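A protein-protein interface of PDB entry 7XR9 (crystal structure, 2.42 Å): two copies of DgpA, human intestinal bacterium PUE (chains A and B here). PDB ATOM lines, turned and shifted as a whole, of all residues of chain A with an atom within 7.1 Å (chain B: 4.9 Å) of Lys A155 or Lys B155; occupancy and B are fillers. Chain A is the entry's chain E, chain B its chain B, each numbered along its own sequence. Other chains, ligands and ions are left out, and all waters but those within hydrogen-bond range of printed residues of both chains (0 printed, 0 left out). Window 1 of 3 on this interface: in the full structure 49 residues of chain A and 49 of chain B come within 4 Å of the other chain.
Tyr A153 touches Glu B253, and with the chains exchanged Glu A253 touches Tyr B153.
Lys A155 touches its own counterpart, Lys B155.
Lys A155 touches Glu B253, and with the chains exchanged Glu A253 touches Lys B155.
12 positions are printed for both chains.
Of the 6 pairs that touch across the chains among the printed residues, 5 have their exchanged pair printed and touching as well.
The backbone carbonyl oxygen (O) of Tyr A153 lies within hydrogen-bond range of the backbone NH (N) of Cys A271.
The backbone NH (N) of Glu B253 lies within hydrogen-bond range of the backbone carbonyl oxygen (O) of Ala B156 (3.0 Å).
The side-chain hydroxyl (OG1) of Thr B268 sits at hydrogen-bond distance from the backbone carbonyl oxygen (O) of Lys B155 (2.9 Å).
The backbone NH (N) of Glu A253 lies within hydrogen-bond range of the backbone carbonyl oxygen (O) of Ala A156 (3.0 Å).
O of Thr A269 is in hydrogen-bond range of N of Lys A155 (2.7 Å).
The side-chain hydroxyl of Thr A268 lies within hydrogen-bond range of the backbone carbonyl oxygen of Lys A155 (3.2 Å).
OH of Tyr A153 is in hydrogen-bond range of OE2 of Glu B253, 2.8 Å away.
The side-chain carboxylate (OE2) of Glu A253 lies within salt-bridge range of the side-chain amino group (NZ) of Lys B155, 3.7 Å away.
OE2 of Glu B253 lies within salt-bridge range of NZ of Lys A155 (3.0 Å).
OH of Tyr B153 sits at hydrogen-bond distance from OE2 of Glu A253, at 2.7 Å.
Of the 22 printed residues of chain A, 4 touch a printed residue of chain B.
Hydrophobic or aromatic side chains of chain A within 4 Å of the printed part of chain B: Tyr A153.
Of the 12 printed residues of chain B, 4 touch a printed residue of chain A.
Printed residues of chain B that touch a printed residue of chain A: Tyr B153, Lys B155, Glu B253 and Met B260.
Among the printed residues, 6 pairs touch across the chains.
Among the printed residues, Asp or Glu carboxylates within 4 Å of a Lys or Arg side-chain nitrogen of the other chain: Lys A155 with Glu B253 (3.0 Å) and Glu A253 with Lys B155 (3.7 Å).
Of the printed residues of chain B, Tyr A153 touches Glu B253 (2.8 Å).
Lys A155 touches just these residues of chain B: Lys B155 (3.7 Å) and Glu B253 (2.9 Å).
Of the printed residues of chain B, Glu A253 touches Tyr B153 (2.7 Å) and Lys B155 (3.0 Å).
Ser A267 touches none of the printed residues of chain B.
Thr A269 touches none of the printed residues of chain B.
Printed residues of chain B within 4 Å of Cys A271: Met B260 (3.9 Å).
Of the printed residues of chain A, Tyr B153 touches Glu A253.
Lys B155 touches just these residues of chain A: Lys A155 and Glu A253.
The nearest residue of chain A that does not touch Lys B155 is Met A260 (5.2 Å).
The nearest printed residue of chain B that does not touch Cys A271 is Glu B253 (7.8 Å).
Among the printed residues, pairs that only touch across the chains: Lys A155 with Lys B155 (3.7 Å) and Cys A271 with Met B260 (3.9 Å).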
ATOM      1  N   ILE A 151      -8.444  21.457  -0.832  1.00  0.00           N
ATOM      2  CA  ILE A 151      -9.166  21.229  -2.076  1.00  0.00           C
ATOM      3  C   ILE A 151      -8.657  19.929  -2.684  1.00  0.00           C
ATOM      4  O   ILE A 151      -7.476  19.818  -3.024  1.00  0.00           O
ATOM      5  CB  ILE A 151      -8.986  22.404  -3.042  1.00  0.00           C
ATOM      6  CG1 ILE A 151      -9.567  23.670  -2.424  1.00  0.00           C
ATOM      7  CG2 ILE A 151      -9.679  22.110  -4.361  1.00  0.00           C
ATOM      8  CD1 ILE A 151      -8.628  24.844  -2.418  1.00  0.00           C
ATOM      9  N   TYR A 153     -10.680  18.163  -5.178  1.00  0.00           N
ATOM     10  CA  TYR A 153     -11.202  18.016  -6.527  1.00  0.00           C
ATOM     11  C   TYR A 153     -11.477  19.401  -7.086  1.00  0.00           C
ATOM     12  O   TYR A 153     -12.201  20.186  -6.467  1.00  0.00           O
ATOM     13  CB  TYR A 153     -12.468  17.167  -6.542  1.00  0.00           C
ATOM     14  CG  TYR A 153     -13.053  17.012  -7.924  1.00  0.00           C
ATOM     15  CD1 TYR A 153     -12.242  16.721  -9.013  1.00  0.00           C
ATOM     16  CD2 TYR A 153     -14.408  17.175  -8.144  1.00  0.00           C
ATOM     17  CE1 TYR A 153     -12.767  16.590 -10.275  1.00  0.00           C
ATOM     18  CE2 TYR A 153     -14.946  17.040  -9.398  1.00  0.00           C
ATOM     19  CZ  TYR A 153     -14.122  16.748 -10.459  1.00  0.00           C
ATOM     20  OH  TYR A 153     -14.668  16.622 -11.710  1.00  0.00           O
ATOM     21  N   GLY A 154     -10.901  19.692  -8.253  1.00  0.00           N
ATOM     22  CA  GLY A 154     -11.103  20.964  -8.904  1.00  0.00           C
ATOM     23  C   GLY A 154     -11.439  20.769 -10.368  1.00  0.00           C
ATOM     24  O   GLY A 154     -11.164  19.725 -10.962  1.00  0.00           O
ATOM     25  N   LYS A 155     -12.051  21.799 -10.950  1.00  0.00           N
ATOM     26  CA  LYS A 155     -12.464  21.745 -12.344  1.00  0.00           C
ATOM     27  C   LYS A 155     -12.056  23.030 -13.038  1.00  0.00           C
ATOM     28  O   LYS A 155     -12.391  24.123 -12.575  1.00  0.00           O
ATOM     29  CB  LYS A 155     -13.976  21.531 -12.477  1.00  0.00           C
ATOM     30  CG  LYS A 155     -14.434  20.153 -12.039  1.00  0.00           C
ATOM     31  CD  LYS A 155     -15.950  20.068 -11.918  1.00  0.00           C
ATOM     32  CE  LYS A 155     -16.579  19.532 -13.194  1.00  0.00           C
ATOM     33  NZ  LYS A 155     -18.060  19.691 -13.184  1.00  0.00           N
ATOM     34  N   ALA A 156     -11.327  22.899 -14.137  1.00  0.00           N
ATOM     35  CA  ALA A 156     -10.976  24.033 -14.980  1.00  0.00           C
ATOM     36  C   ALA A 156     -11.969  24.101 -16.136  1.00  0.00           C
ATOM     37  O   ALA A 156     -12.052  23.166 -16.942  1.00  0.00           O
ATOM     38  CB  ALA A 156      -9.544  23.900 -15.499  1.00  0.00           C
ATOM     39  N   HIS A 157     -12.722  25.196 -16.211  1.00  0.00           N
ATOM     40  CA  HIS A 157     -13.752  25.381 -17.227  1.00  0.00           C
ATOM     41  C   HIS A 157     -13.242  26.351 -18.287  1.00  0.00           C
ATOM     42  O   HIS A 157     -12.955  27.513 -17.981  1.00  0.00           O
ATOM     43  CB  HIS A 157     -15.048  25.905 -16.609  1.00  0.00           C
ATOM     44  CG  HIS A 157     -15.740  24.921 -15.720  1.00  0.00           C
ATOM     45  ND1 HIS A 157     -16.560  23.924 -16.205  1.00  0.00           N
ATOM     46  CD2 HIS A 157     -15.750  24.792 -14.371  1.00  0.00           C
ATOM     47  CE1 HIS A 157     -17.036  23.217 -15.195  1.00  0.00           C
ATOM     48  NE2 HIS A 157     -16.556  23.719 -14.072  1.00  0.00           N
ATOM     49  N   ALA A 188      -8.234  28.937 -17.553  1.00  0.00           N
ATOM     50  CA  ALA A 188      -8.999  28.169 -16.577  1.00  0.00           C
ATOM     51  C   ALA A 188      -8.096  27.331 -15.680  1.00  0.00           C
ATOM     52  O   ALA A 188      -8.334  27.234 -14.471  1.00  0.00           O
ATOM     53  CB  ALA A 188     -10.011  27.277 -17.292  1.00  0.00           C
ATOM     54  N   LEU A 189      -7.063  26.705 -16.249  1.00  0.00           N
ATOM     55  CA  LEU A 189      -6.203  25.853 -15.432  1.00  0.00           C
ATOM     56  C   LEU A 189      -5.296  26.675 -14.531  1.00  0.00           C
ATOM     57  O   LEU A 189      -5.035  26.278 -13.391  1.00  0.00           O
ATOM     58  CB  LEU A 189      -5.369  24.925 -16.316  1.00  0.00           C
ATOM     59  CG  LEU A 189      -4.488  23.935 -15.553  1.00  0.00           C
ATOM     60  CD1 LEU A 189      -5.276  22.719 -15.047  1.00  0.00           C
ATOM     61  CD2 LEU A 189      -3.343  23.490 -16.452  1.00  0.00           C
ATOM     62  N   THR A 192      -7.251  27.553 -11.567  1.00  0.00           N
ATOM     63  CA  THR A 192      -7.539  26.366 -10.774  1.00  0.00           C
ATOM     64  C   THR A 192      -6.330  25.936  -9.955  1.00  0.00           C
ATOM     65  O   THR A 192      -6.456  25.617  -8.767  1.00  0.00           O
ATOM     66  CB  THR A 192      -8.000  25.235 -11.690  1.00  0.00           C
ATOM     67  OG1 THR A 192      -9.134  25.682 -12.433  1.00  0.00           O
ATOM     68  CG2 THR A 192      -8.388  24.009 -10.874  1.00  0.00           C
ATOM     69  N   MET A 196      -5.909  26.311  -5.765  1.00  0.00           N
ATOM     70  CA  MET A 196      -5.582  25.098  -5.028  1.00  0.00           C
ATOM     71  C   MET A 196      -4.185  25.146  -4.429  1.00  0.00           C
ATOM     72  O   MET A 196      -3.892  24.362  -3.521  1.00  0.00           O
ATOM     73  CB  MET A 196      -5.699  23.879  -5.940  1.00  0.00           C
ATOM     74  CG  MET A 196      -7.116  23.572  -6.356  1.00  0.00           C
ATOM     75  SD  MET A 196      -7.198  22.181  -7.475  1.00  0.00           S
ATOM     76  CE  MET A 196      -6.522  20.866  -6.451  1.00  0.00           C
ATOM     77  N   THR A 249      -7.422  15.893  -7.574  1.00  0.00           N
ATOM     78  CA  THR A 249      -7.708  15.687  -8.991  1.00  0.00           C
ATOM     79  C   THR A 249      -8.313  16.943  -9.607  1.00  0.00           C
ATOM     80  O   THR A 249      -9.146  17.610  -8.983  1.00  0.00           O
ATOM     81  CB  THR A 249      -8.670  14.498  -9.190  1.00  0.00           C
ATOM     82  OG1 THR A 249      -8.055  13.292  -8.717  1.00  0.00           O
ATOM     83  CG2 THR A 249      -9.021  14.324 -10.654  1.00  0.00           C
ATOM     84  N   ILE A 250      -7.908  17.257 -10.839  1.00  0.00           N
ATOM     85  CA  ILE A 250      -8.439  18.396 -11.587  1.00  0.00           C
ATOM     86  C   ILE A 250      -8.978  17.895 -12.916  1.00  0.00           C
ATOM     87  O   ILE A 250      -8.226  17.331 -13.719  1.00  0.00           O
ATOM     88  CB  ILE A 250      -7.382  19.481 -11.830  1.00  0.00           C
ATOM     89  CG1 ILE A 250      -7.019  20.193 -10.531  1.00  0.00           C
ATOM     90  CG2 ILE A 250      -7.903  20.475 -12.856  1.00  0.00           C
ATOM     91  CD1 ILE A 250      -5.535  20.358 -10.325  1.00  0.00           C
ATOM     92  N   GLY A 251     -10.268  18.108 -13.153  1.00  0.00           N
ATOM     93  CA  GLY A 251     -10.845  17.897 -14.470  1.00  0.00           C
ATOM     94  C   GLY A 251     -10.779  19.184 -15.278  1.00  0.00           C
ATOM     95  O   GLY A 251     -10.885  20.282 -14.734  1.00  0.00           O
ATOM     96  N   LEU A 252     -10.596  19.036 -16.588  1.00  0.00           N
ATOM     97  CA  LEU A 252     -10.431  20.177 -17.476  1.00  0.00           C
ATOM     98  C   LEU A 252     -11.320  20.012 -18.700  1.00  0.00           C
ATOM     99  O   LEU A 252     -11.412  18.920 -19.267  1.00  0.00           O
ATOM    100  CB  LEU A 252      -8.967  20.321 -17.898  1.00  0.00           C
ATOM    101  CG  LEU A 252      -8.518  21.589 -18.622  1.00  0.00           C
ATOM    102  CD1 LEU A 252      -7.106  21.961 -18.187  1.00  0.00           C
ATOM    103  CD2 LEU A 252      -8.572  21.376 -20.122  1.00  0.00           C
ATOM    104  N   GLU A 253     -11.972  21.101 -19.107  1.00  0.00           N
ATOM    105  CA  GLU A 253     -12.769  21.117 -20.327  1.00  0.00           C
ATOM    106  C   GLU A 253     -12.470  22.398 -21.081  1.00  0.00           C
ATOM    107  O   GLU A 253     -12.499  23.485 -20.497  1.00  0.00           O
ATOM    108  CB  GLU A 253     -14.266  21.020 -20.031  1.00  0.00           C
ATOM    109  CG  GLU A 253     -14.691  19.678 -19.469  1.00  0.00           C
ATOM    110  CD  GLU A 253     -16.124  19.685 -18.985  1.00  0.00           C
ATOM    111  OE1 GLU A 253     -16.713  20.784 -18.879  1.00  0.00           O
ATOM    112  OE2 GLU A 253     -16.662  18.593 -18.702  1.00  0.00           O
ATOM    113  N   MET A 260     -22.571  21.641 -26.154  1.00  0.00           N
ATOM    114  CA  MET A 260     -22.854  21.708 -24.733  1.00  0.00           C
ATOM    115  C   MET A 260     -23.495  23.054 -24.429  1.00  0.00           C
ATOM    116  O   MET A 260     -23.157  24.079 -25.039  1.00  0.00           O
ATOM    117  CB  MET A 260     -21.582  21.544 -23.917  1.00  0.00           C
ATOM    118  CG  MET A 260     -21.683  20.560 -22.798  1.00  0.00           C
ATOM    119  SD  MET A 260     -20.041  20.301 -22.117  1.00  0.00           S
ATOM    120  CE  MET A 260     -19.712  21.941 -21.476  1.00  0.00           C
ATOM    121  N   ARG A 264     -18.844  28.380 -20.516  1.00  0.00           N
ATOM    122  CA  ARG A 264     -18.190  28.787 -19.279  1.00  0.00           C
ATOM    123  C   ARG A 264     -16.684  28.712 -19.480  1.00  0.00           C
ATOM    124  O   ARG A 264     -16.152  27.634 -19.763  1.00  0.00           O
ATOM    125  CB  ARG A 264     -18.633  27.895 -18.109  1.00  0.00           C
ATOM    126  CG  ARG A 264     -18.631  28.606 -16.762  1.00  0.00           C
ATOM    127  CD  ARG A 264     -18.688  27.630 -15.607  1.00  0.00           C
ATOM    128  NE  ARG A 264     -20.021  27.067 -15.430  1.00  0.00           N
ATOM    129  CZ  ARG A 264     -20.365  26.269 -14.424  1.00  0.00           C
ATOM    130  NH1 ARG A 264     -19.477  25.937 -13.501  1.00  0.00           N
ATOM    131  NH2 ARG A 264     -21.601  25.806 -14.339  1.00  0.00           N
ATOM    132  N   SER A 267     -13.179  30.113 -15.741  1.00  0.00           N
ATOM    133  CA  SER A 267     -13.911  29.823 -14.523  1.00  0.00           C
ATOM    134  C   SER A 267     -13.336  28.575 -13.871  1.00  0.00           C
ATOM    135  O   SER A 267     -12.601  27.805 -14.499  1.00  0.00           O
ATOM    136  CB  SER A 267     -15.399  29.620 -14.818  1.00  0.00           C
ATOM    137  OG  SER A 267     -15.994  30.823 -15.272  1.00  0.00           O
ATOM    138  N   THR A 268     -13.703  28.361 -12.610  1.00  0.00           N
ATOM    139  CA  THR A 268     -13.186  27.209 -11.888  1.00  0.00           C
ATOM    140  C   THR A 268     -14.225  26.704 -10.899  1.00  0.00           C
ATOM    141  O   THR A 268     -15.138  27.430 -10.496  1.00  0.00           O
ATOM    142  CB  THR A 268     -11.880  27.545 -11.162  1.00  0.00           C
ATOM    143  OG1 THR A 268     -11.409  26.385 -10.468  1.00  0.00           O
ATOM    144  CG2 THR A 268     -12.104  28.672 -10.172  1.00  0.00           C
ATOM    145  N   THR A 269     -14.080  25.438 -10.523  1.00  0.00           N
ATOM    146  CA  THR A 269     -14.885  24.823  -9.481  1.00  0.00           C
ATOM    147  C   THR A 269     -13.932  24.133  -8.522  1.00  0.00           C
ATOM    148  O   THR A 269     -13.039  23.402  -8.963  1.00  0.00           O
ATOM    149  CB  THR A 269     -15.884  23.816 -10.061  1.00  0.00           C
ATOM    150  OG1 THR A 269     -16.682  24.453 -11.070  1.00  0.00           O
ATOM    151  CG2 THR A 269     -16.793  23.258  -8.965  1.00  0.00           C
ATOM    152  N   LEU A 270     -14.112  24.382  -7.223  1.00  0.00           N
ATOM    153  CA  LEU A 270     -13.233  23.876  -6.174  1.00  0.00           C
ATOM    154  C   LEU A 270     -14.075  23.216  -5.090  1.00  0.00           C
ATOM    155  O   LEU A 270     -15.012  23.826  -4.565  1.00  0.00           O
ATOM    156  CB  LEU A 270     -12.387  25.007  -5.575  1.00  0.00           C
ATOM    157  CG  LEU A 270     -11.608  25.931  -6.510  1.00  0.00           C
ATOM    158  CD1 LEU A 270     -10.647  26.817  -5.711  1.00  0.00           C
ATOM    159  CD2 LEU A 270     -10.851  25.099  -7.511  1.00  0.00           C
ATOM    160  N   CYS A 271     -13.745  21.970  -4.776  1.00  0.00           N
ATOM    161  CA  CYS A 271     -14.398  21.413  -3.598  1.00  0.00           C
ATOM    162  C   CYS A 271     -13.306  21.054  -2.601  1.00  0.00           C
ATOM    163  O   CYS A 271     -12.410  20.274  -2.928  1.00  0.00           O
ATOM    164  CB  CYS A 271     -15.226  20.178  -3.952  1.00  0.00           C
ATOM    165  SG  CYS A 271     -16.346  20.346  -5.370  1.00  0.00           S
ATOM    166  N   TYR B 153     -18.198  12.926 -26.492  1.00  0.00           N
ATOM    167  CA  TYR B 153     -17.990  13.321 -25.109  1.00  0.00           C
ATOM    168  C   TYR B 153     -19.287  13.133 -24.350  1.00  0.00           C
ATOM    169  O   TYR B 153     -20.332  13.653 -24.754  1.00  0.00           O
ATOM    170  CB  TYR B 153     -17.505  14.768 -24.982  1.00  0.00           C
ATOM    171  CG  TYR B 153     -17.117  15.134 -23.559  1.00  0.00           C
ATOM    172  CD1 TYR B 153     -16.369  14.261 -22.774  1.00  0.00           C
ATOM    173  CD2 TYR B 153     -17.505  16.348 -22.997  1.00  0.00           C
ATOM    174  CE1 TYR B 153     -16.010  14.590 -21.468  1.00  0.00           C
ATOM    175  CE2 TYR B 153     -17.153  16.686 -21.688  1.00  0.00           C
ATOM    176  CZ  TYR B 153     -16.407  15.805 -20.932  1.00  0.00           C
ATOM    177  OH  TYR B 153     -16.058  16.141 -19.640  1.00  0.00           O
ATOM    178  N   GLY B 154     -19.216  12.373 -23.267  1.00  0.00           N
ATOM    179  CA  GLY B 154     -20.351  12.184 -22.393  1.00  0.00           C
ATOM    180  C   GLY B 154     -19.927  12.399 -20.959  1.00  0.00           C
ATOM    181  O   GLY B 154     -18.769  12.198 -20.596  1.00  0.00           O
ATOM    182  N   LYS B 155     -20.889  12.831 -20.145  1.00  0.00           N
ATOM    183  CA  LYS B 155     -20.673  13.029 -18.719  1.00  0.00           C
ATOM    184  C   LYS B 155     -21.758  12.297 -17.955  1.00  0.00           C
ATOM    185  O   LYS B 155     -22.951  12.517 -18.197  1.00  0.00           O
ATOM    186  CB  LYS B 155     -20.685  14.516 -18.339  1.00  0.00           C
ATOM    187  CG  LYS B 155     -19.457  15.290 -18.761  1.00  0.00           C
ATOM    188  CD  LYS B 155     -19.588  16.760 -18.390  1.00  0.00           C
ATOM    189  CE  LYS B 155     -18.782  17.080 -17.143  1.00  0.00           C
ATOM    190  NZ  LYS B 155     -19.405  18.164 -16.328  1.00  0.00           N
ATOM    191  N   ALA B 156     -21.350  11.430 -17.043  1.00  0.00           N
ATOM    192  CA  ALA B 156     -22.270  10.787 -16.116  1.00  0.00           C
ATOM    193  C   ALA B 156     -22.293  11.604 -14.831  1.00  0.00           C
ATOM    194  O   ALA B 156     -21.263  11.750 -14.159  1.00  0.00           O
ATOM    195  CB  ALA B 156     -21.862   9.343 -15.839  1.00  0.00           C
ATOM    196  N   HIS B 157     -23.461  12.139 -14.500  1.00  0.00           N
ATOM    197  CA  HIS B 157     -23.651  12.954 -13.309  1.00  0.00           C
ATOM    198  C   HIS B 157     -24.321  12.115 -12.228  1.00  0.00           C
ATOM    199  O   HIS B 157     -25.453  11.645 -12.411  1.00  0.00           O
ATOM    200  CB  HIS B 157     -24.496  14.184 -13.626  1.00  0.00           C
ATOM    201  CG  HIS B 157     -23.865  15.114 -14.610  1.00  0.00           C
ATOM    202  ND1 HIS B 157     -22.664  15.745 -14.369  1.00  0.00           N
ATOM    203  CD2 HIS B 157     -24.270  15.529 -15.832  1.00  0.00           C
ATOM    204  CE1 HIS B 157     -22.354  16.509 -15.402  1.00  0.00           C
ATOM    205  NE2 HIS B 157     -23.313  16.396 -16.304  1.00  0.00           N
ATOM    206  N   THR B 192     -25.689   6.886 -19.406  1.00  0.00           N
ATOM    207  CA  THR B 192     -24.706   7.452 -20.329  1.00  0.00           C
ATOM    208  C   THR B 192     -24.253   6.427 -21.366  1.00  0.00           C
ATOM    209  O   THR B 192     -24.293   6.696 -22.574  1.00  0.00           O
ATOM    210  CB  THR B 192     -23.501   7.998 -19.557  1.00  0.00           C
ATOM    211  OG1 THR B 192     -23.885   9.158 -18.805  1.00  0.00           O
ATOM    212  CG2 THR B 192     -22.390   8.382 -20.511  1.00  0.00           C
ATOM    213  N   GLY B 251     -16.738  11.241 -18.767  1.00  0.00           N
ATOM    214  CA  GLY B 251     -16.421  11.650 -17.414  1.00  0.00           C
ATOM    215  C   GLY B 251     -17.542  11.265 -16.462  1.00  0.00           C
ATOM    216  O   GLY B 251     -18.718  11.296 -16.812  1.00  0.00           O
ATOM    217  N   GLU B 253     -18.887  11.743 -12.330  1.00  0.00           N
ATOM    218  CA  GLU B 253     -18.799  12.329 -10.993  1.00  0.00           C
ATOM    219  C   GLU B 253     -19.849  11.663 -10.125  1.00  0.00           C
ATOM    220  O   GLU B 253     -21.043  11.723 -10.440  1.00  0.00           O
ATOM    221  CB  GLU B 253     -19.018  13.844 -11.005  1.00  0.00           C
ATOM    222  CG  GLU B 253     -17.845  14.658 -11.517  1.00  0.00           C
ATOM    223  CD  GLU B 253     -18.263  16.046 -11.971  1.00  0.00           C
ATOM    224  OE1 GLU B 253     -19.479  16.313 -12.039  1.00  0.00           O
ATOM    225  OE2 GLU B 253     -17.378  16.874 -12.257  1.00  0.00           O
ATOM    226  N   MET B 260     -20.146  20.933  -3.288  1.00  0.00           N
ATOM    227  CA  MET B 260     -20.418  21.310  -4.665  1.00  0.00           C
ATOM    228  C   MET B 260     -21.856  21.800  -4.759  1.00  0.00           C
ATOM    229  O   MET B 260     -22.749  21.264  -4.095  1.00  0.00           O
ATOM    230  CB  MET B 260     -20.186  20.114  -5.607  1.00  0.00           C
ATOM    231  CG  MET B 260     -19.960  20.474  -7.056  1.00  0.00           C
ATOM    232  SD  MET B 260     -19.094  19.155  -7.936  1.00  0.00           S
ATOM    233  CE  MET B 260     -19.816  19.348  -9.572  1.00  0.00           C
ATOM    234  N   SER B 267     -28.223  11.497 -14.111  1.00  0.00           N
ATOM    235  CA  SER B 267     -28.268  12.458 -15.197  1.00  0.00           C
ATOM    236  C   SER B 267     -27.085  12.220 -16.120  1.00  0.00           C
ATOM    237  O   SER B 267     -26.043  11.699 -15.709  1.00  0.00           O
ATOM    238  CB  SER B 267     -28.228  13.895 -14.669  1.00  0.00           C
ATOM    239  OG  SER B 267     -29.273  14.136 -13.740  1.00  0.00           O
ATOM    240  N   THR B 268     -27.254  12.618 -17.378  1.00  0.00           N
ATOM    241  CA  THR B 268     -26.117  12.535 -18.275  1.00  0.00           C
ATOM    242  C   THR B 268     -26.116  13.749 -19.187  1.00  0.00           C
ATOM    243  O   THR B 268     -27.156  14.364 -19.434  1.00  0.00           O
ATOM    244  CB  THR B 268     -26.128  11.238 -19.119  1.00  0.00           C
ATOM    245  OG1 THR B 268     -24.901  11.130 -19.854  1.00  0.00           O
ATOM    246  CG2 THR B 268     -27.275  11.243 -20.108  1.00  0.00           C
ATOM    247  N   THR B 269     -24.933  13.967 -19.751  1.00  0.00           N
ATOM    248  CA  THR B 269     -24.654  15.072 -20.655  1.00  0.00           C
ATOM    249  C   THR B 269     -23.946  14.490 -21.864  1.00  0.00           C
ATOM    250  O   THR B 269     -22.903  13.845 -21.724  1.00  0.00           O
ATOM    251  CB  THR B 269     -23.785  16.143 -19.990  1.00  0.00           C
ATOM    252  OG1 THR B 269     -24.510  16.757 -18.920  1.00  0.00           O
ATOM    253  CG2 THR B 269     -23.379  17.209 -21.003  1.00  0.00           C
